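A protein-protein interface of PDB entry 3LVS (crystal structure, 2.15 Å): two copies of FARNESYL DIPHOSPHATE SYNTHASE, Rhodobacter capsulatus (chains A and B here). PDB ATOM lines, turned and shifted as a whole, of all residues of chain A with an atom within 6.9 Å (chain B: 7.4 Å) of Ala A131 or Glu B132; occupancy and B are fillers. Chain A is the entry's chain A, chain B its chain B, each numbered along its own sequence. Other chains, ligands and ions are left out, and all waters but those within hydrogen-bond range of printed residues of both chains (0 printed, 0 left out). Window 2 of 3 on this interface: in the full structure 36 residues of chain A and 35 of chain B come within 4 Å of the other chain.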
ATOM      1  N   GLY A 129       2.242 -23.732  20.190  1.00  0.00           N
ATOM      2  CA  GLY A 129       2.012 -22.570  21.041  1.00  0.00           C
ATOM      3  C   GLY A 129       2.935 -22.540  22.234  1.00  0.00           C
ATOM      4  O   GLY A 129       4.065 -23.030  22.151  1.00  0.00           O
ATOM      5  N   SER A 130       2.443 -21.987  23.344  1.00  0.00           N
ATOM      6  CA  SER A 130       3.260 -21.712  24.529  1.00  0.00           C
ATOM      7  C   SER A 130       3.864 -22.970  25.141  1.00  0.00           C
ATOM      8  O   SER A 130       3.306 -24.061  25.015  1.00  0.00           O
ATOM      9  CB  SER A 130       2.444 -20.978  25.594  1.00  0.00           C
ATOM     10  OG  SER A 130       1.939 -21.879  26.572  1.00  0.00           O
ATOM     11  N   ALA A 131       4.996 -22.795  25.815  1.00  0.00           N
ATOM     12  CA  ALA A 131       5.700 -23.896  26.471  1.00  0.00           C
ATOM     13  C   ALA A 131       4.927 -24.446  27.659  1.00  0.00           C
ATOM     14  O   ALA A 131       5.133 -25.604  28.053  1.00  0.00           O
ATOM     15  CB  ALA A 131       7.096 -23.456  26.908  1.00  0.00           C
ATOM     16  N   GLU A 132       4.064 -23.605  28.234  1.00  0.00           N
ATOM     17  CA  GLU A 132       3.195 -24.005  29.336  1.00  0.00           C
ATOM     18  C   GLU A 132       2.207 -25.070  28.866  1.00  0.00           C
ATOM     19  O   GLU A 132       2.051 -26.114  29.501  1.00  0.00           O
ATOM     20  CB  GLU A 132       2.448 -22.793  29.900  1.00  0.00           C
ATOM     21  CG  GLU A 132       1.795 -23.039  31.248  1.00  0.00           C
ATOM     22  CD  GLU A 132       2.811 -23.279  32.345  1.00  0.00           C
ATOM     23  OE1 GLU A 132       2.564 -24.142  33.211  1.00  0.00           O
ATOM     24  OE2 GLU A 132       3.862 -22.604  32.341  1.00  0.00           O
ATOM     25  N   ASN A 133       1.557 -24.799  27.737  1.00  0.00           N
ATOM     26  CA  ASN A 133       0.583 -25.724  27.159  1.00  0.00           C
ATOM     27  C   ASN A 133       1.248 -26.988  26.612  1.00  0.00           C
ATOM     28  O   ASN A 133       0.702 -28.093  26.743  1.00  0.00           O
ATOM     29  CB  ASN A 133      -0.236 -25.023  26.072  1.00  0.00           C
ATOM     30  CG  ASN A 133      -1.113 -23.907  26.624  1.00  0.00           C
ATOM     31  OD1 ASN A 133      -1.421 -23.866  27.815  1.00  0.00           O
ATOM     32  ND2 ASN A 133      -1.523 -23.004  25.753  1.00  0.00           N
ATOM     33  N   ARG A 134       2.435 -26.812  26.028  1.00  0.00           N
ATOM     34  CA  ARG A 134       3.234 -27.927  25.534  1.00  0.00           C
ATOM     35  C   ARG A 134       3.654 -28.877  26.654  1.00  0.00           C
ATOM     36  O   ARG A 134       3.614 -30.085  26.477  1.00  0.00           O
ATOM     37  CB  ARG A 134       4.451 -27.438  24.743  1.00  0.00           C
ATOM     38  CG  ARG A 134       4.138 -27.142  23.293  1.00  0.00           C
ATOM     39  CD  ARG A 134       5.364 -26.681  22.545  1.00  0.00           C
ATOM     40  NE  ARG A 134       5.696 -25.301  22.890  1.00  0.00           N
ATOM     41  CZ  ARG A 134       6.907 -24.763  22.793  1.00  0.00           C
ATOM     42  NH1 ARG A 134       7.932 -25.482  22.370  1.00  0.00           N
ATOM     43  NH2 ARG A 134       7.093 -23.495  23.132  1.00  0.00           N
ATOM     44  N   VAL A 135       4.008 -28.342  27.814  1.00  0.00           N
ATOM     45  CA  VAL A 135       4.457 -29.218  28.899  1.00  0.00           C
ATOM     46  C   VAL A 135       3.265 -29.978  29.512  1.00  0.00           C
ATOM     47  O   VAL A 135       3.385 -31.150  29.876  1.00  0.00           O
ATOM     48  CB  VAL A 135       5.405 -28.494  29.928  1.00  0.00           C
ATOM     49  CG1 VAL A 135       4.651 -27.554  30.840  1.00  0.00           C
ATOM     50  CG2 VAL A 135       6.182 -29.508  30.764  1.00  0.00           C
ATOM     51  N   ALA A 136       2.108 -29.321  29.547  1.00  0.00           N
ATOM     52  CA  ALA A 136       0.872 -29.953  29.984  1.00  0.00           C
ATOM     53  C   ALA A 136       0.445 -31.026  28.976  1.00  0.00           C
ATOM     54  O   ALA A 136      -0.025 -32.090  29.383  1.00  0.00           O
ATOM     55  CB  ALA A 136      -0.214 -28.924  30.190  1.00  0.00           C
ATOM     56  N   LEU A 137       0.661 -30.760  27.683  1.00  0.00           N
ATOM     57  CA  LEU A 137       0.424 -31.748  26.637  1.00  0.00           C
ATOM     58  C   LEU A 137       1.250 -33.026  26.825  1.00  0.00           C
ATOM     59  O   LEU A 137       0.692 -34.126  26.757  1.00  0.00           O
ATOM     60  CB  LEU A 137       0.671 -31.171  25.257  1.00  0.00           C
ATOM     61  CG  LEU A 137       0.085 -31.947  24.069  1.00  0.00           C
ATOM     62  CD1 LEU A 137      -1.450 -31.904  24.037  1.00  0.00           C
ATOM     63  CD2 LEU A 137       0.634 -31.400  22.771  1.00  0.00           C
ATOM     64  N   GLY B 129      11.706 -26.600  37.214  1.00  0.00           N
ATOM     65  CA  GLY B 129      11.758 -25.167  36.943  1.00  0.00           C
ATOM     66  C   GLY B 129      10.760 -24.788  35.881  1.00  0.00           C
ATOM     67  O   GLY B 129       9.710 -25.412  35.769  1.00  0.00           O
ATOM     68  N   SER B 130      11.099 -23.781  35.082  1.00  0.00           N
ATOM     69  CA  SER B 130      10.184 -23.219  34.090  1.00  0.00           C
ATOM     70  C   SER B 130       9.732 -24.201  33.006  1.00  0.00           C
ATOM     71  O   SER B 130      10.426 -25.180  32.693  1.00  0.00           O
ATOM     72  CB  SER B 130      10.826 -21.995  33.433  1.00  0.00           C
ATOM     73  OG  SER B 130      11.795 -22.392  32.480  1.00  0.00           O
ATOM     74  N   ALA B 131       8.574 -23.904  32.420  1.00  0.00           N
ATOM     75  CA  ALA B 131       8.007 -24.690  31.329  1.00  0.00           C
ATOM     76  C   ALA B 131       8.912 -24.685  30.102  1.00  0.00           C
ATOM     77  O   ALA B 131       9.041 -25.699  29.415  1.00  0.00           O
ATOM     78  CB  ALA B 131       6.632 -24.157  30.964  1.00  0.00           C
ATOM     79  N   GLU B 132       9.537 -23.535  29.854  1.00  0.00           N
ATOM     80  CA  GLU B 132      10.453 -23.317  28.732  1.00  0.00           C
ATOM     81  C   GLU B 132      11.645 -24.272  28.768  1.00  0.00           C
ATOM     82  O   GLU B 132      12.052 -24.831  27.743  1.00  0.00           O
ATOM     83  CB  GLU B 132      10.963 -21.884  28.779  1.00  0.00           C
ATOM     84  CG  GLU B 132      11.451 -21.362  27.457  1.00  0.00           C
ATOM     85  CD  GLU B 132      10.306 -21.065  26.516  1.00  0.00           C
ATOM     86  OE1 GLU B 132      10.397 -21.439  25.324  1.00  0.00           O
ATOM     87  OE2 GLU B 132       9.307 -20.467  26.978  1.00  0.00           O
ATOM     88  N   ASN B 133      12.197 -24.441  29.963  1.00  0.00           N
ATOM     89  CA  ASN B 133      13.327 -25.314  30.183  1.00  0.00           C
ATOM     90  C   ASN B 133      12.927 -26.776  30.107  1.00  0.00           C
ATOM     91  O   ASN B 133      13.662 -27.594  29.549  1.00  0.00           O
ATOM     92  CB  ASN B 133      14.003 -24.978  31.524  1.00  0.00           C
ATOM     93  CG  ASN B 133      14.772 -23.657  31.476  1.00  0.00           C
ATOM     94  OD1 ASN B 133      14.902 -23.034  30.418  1.00  0.00           O
ATOM     95  ND2 ASN B 133      15.297 -23.237  32.616  1.00  0.00           N
ATOM     96  N   ARG B 134      11.751 -27.084  30.648  1.00  0.00           N
ATOM     97  CA  ARG B 134      11.205 -28.441  30.665  1.00  0.00           C
ATOM     98  C   ARG B 134      10.910 -28.962  29.265  1.00  0.00           C
ATOM     99  O   ARG B 134      11.184 -30.116  28.968  1.00  0.00           O
ATOM    100  CB  ARG B 134       9.959 -28.511  31.557  1.00  0.00           C
ATOM    101  CG  ARG B 134      10.296 -28.696  33.032  1.00  0.00           C
ATOM    102  CD  ARG B 134       9.060 -28.738  33.902  1.00  0.00           C
ATOM    103  NE  ARG B 134       8.386 -27.442  33.933  1.00  0.00           N
ATOM    104  CZ  ARG B 134       7.140 -27.238  34.348  1.00  0.00           C
ATOM    105  NH1 ARG B 134       6.384 -28.239  34.780  1.00  0.00           N
ATOM    106  NH2 ARG B 134       6.648 -26.015  34.326  1.00  0.00           N
ATOM    107  N   VAL B 135      10.396 -28.090  28.400  1.00  0.00           N
ATOM    108  CA  VAL B 135      10.091 -28.468  27.033  1.00  0.00           C
ATOM    109  C   VAL B 135      11.363 -28.633  26.175  1.00  0.00           C
ATOM    110  O   VAL B 135      11.390 -29.441  25.244  1.00  0.00           O
ATOM    111  CB  VAL B 135       8.995 -27.528  26.401  1.00  0.00           C
ATOM    112  CG1 VAL B 135       9.568 -26.241  25.882  1.00  0.00           C
ATOM    113  CG2 VAL B 135       8.238 -28.237  25.312  1.00  0.00           C
ATOM    114  N   ALA B 136      12.422 -27.895  26.510  1.00  0.00           N
ATOM    115  CA  ALA B 136      13.724 -28.108  25.889  1.00  0.00           C
ATOM    116  C   ALA B 136      14.342 -29.422  26.379  1.00  0.00           C
ATOM    117  O   ALA B 136      15.048 -30.106  25.644  1.00  0.00           O
ATOM    118  CB  ALA B 136      14.660 -26.929  26.171  1.00  0.00           C
ATOM    119  N   LEU B 137      14.067 -29.772  27.624  1.00  0.00           N
ATOM    120  CA  LEU B 137      14.584 -31.016  28.201  1.00  0.00           C
ATOM    121  C   LEU B 137      13.934 -32.271  27.573  1.00  0.00           C
ATOM    122  O   LEU B 137      14.629 -33.244  27.258  1.00  0.00           O
ATOM    123  CB  LEU B 137      14.410 -30.987  29.720  1.00  0.00           C
ATOM    124  CG  LEU B 137      15.130 -32.077  30.525  1.00  0.00           C
ATOM    125  CD1 LEU B 137      16.592 -31.701  30.723  1.00  0.00           C
ATOM    126  CD2 LEU B 137      14.451 -32.274  31.862  1.00  0.00           C
ATOM    127  N   ILE B 193      20.609 -27.135  30.377  1.00  0.00           N
ATOM    128  CA  ILE B 193      19.239 -27.029  29.875  1.00  0.00           C
ATOM    129  C   ILE B 193      18.339 -26.419  30.957  1.00  0.00           C
ATOM    130  O   ILE B 193      17.571 -25.481  30.689  1.00  0.00           O
ATOM    131  CB  ILE B 193      18.705 -28.405  29.365  1.00  0.00           C
ATOM    132  CG1 ILE B 193      19.446 -28.825  28.084  1.00  0.00           C
ATOM    133  CG2 ILE B 193      17.195 -28.363  29.092  1.00  0.00           C
ATOM    134  CD1 ILE B 193      19.116 -30.238  27.563  1.00  0.00           C
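O of Gly A129 sits at hydrogen-bond distance from NE of Arg A134 (2.9 Å).
N of Glu A132 sits close to OG of Ser A130.
The guanidinium group of Arg A134 sits at hydrogen-bond distance from the backbone carbonyl oxygen of Ser A130, at 3.4 Å.
The backbone carbonyl oxygen (O) of Gly B129 sits at hydrogen-bond distance from the guanidinium group (NE) of Arg B134 (3.0 Å).
The backbone carbonyl oxygen of Ser B130 is in hydrogen-bond range of the guanidinium group of Arg B134, at 3.3 Å.
O of Ala A131 touches CB of Ala B131 (3.6 Å).
Glu B132 touches Ala A131.
Val B135 touches Ala A131.
Ala B131 touches Glu A132 (CB to OE2, 3.5 Å).
CB of Arg A134 touches CG2 of Val B135, 3.9 Å away.
Val A135 touches Ala B131.
CB of Arg B134 touches CG2 of Val A135, 3.99 Å away.
Of chain B, only Ala B131, Glu B132 and Val B135 come within 4 Å of Ala A131.
Printed residues of chain B within 4 Å of Glu A132: Ala B131.
Asn A133 touches none of the printed residues of chain B.
Of the printed residues of chain B, Val A135 touches Ala B131 (3.9 Å) and Arg B134 (3.99 Å).
Of chain A, only Ala A131 (3.7 Å) comes within 4 Å of Glu B132.
Of the printed residues of chain A, Arg B134 touches Val A135.
The nearest residue of chain B that does not touch Ala A131 is Asn B133 (6.0 Å).
The nearest printed residue of chain A that does not touch Arg B134 is Glu A132 (4.6 Å).
Printed residues of chain A that touch a printed residue of chain B: Ala A131, Glu A132, Arg A134 and Val A135.
Hydrophobic or aromatic side chains of chain A within 4 Å of the printed part of chain B: Ala A131 and Val A135.
Hydrophobic or aromatic side chains of chain B within 4 Å of the printed part of chain A: Ala B131 and Val B135.
Ala B131 touches its own counterpart, Ala A131.
Ala A131 touches Glu B132, and with the chains exchanged Glu A132 touches Ala B131.
Ala A131 touches Val B135, and with the chains exchanged Val A135 touches Ala B131.
Arg A134 touches Val B135, and with the chains exchanged Val A135 touches Arg B134.
9 positions are printed for both chains.
Of the 7 pairs that touch across the chains among the printed residues, 7 have their exchanged pair printed and touching as well.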
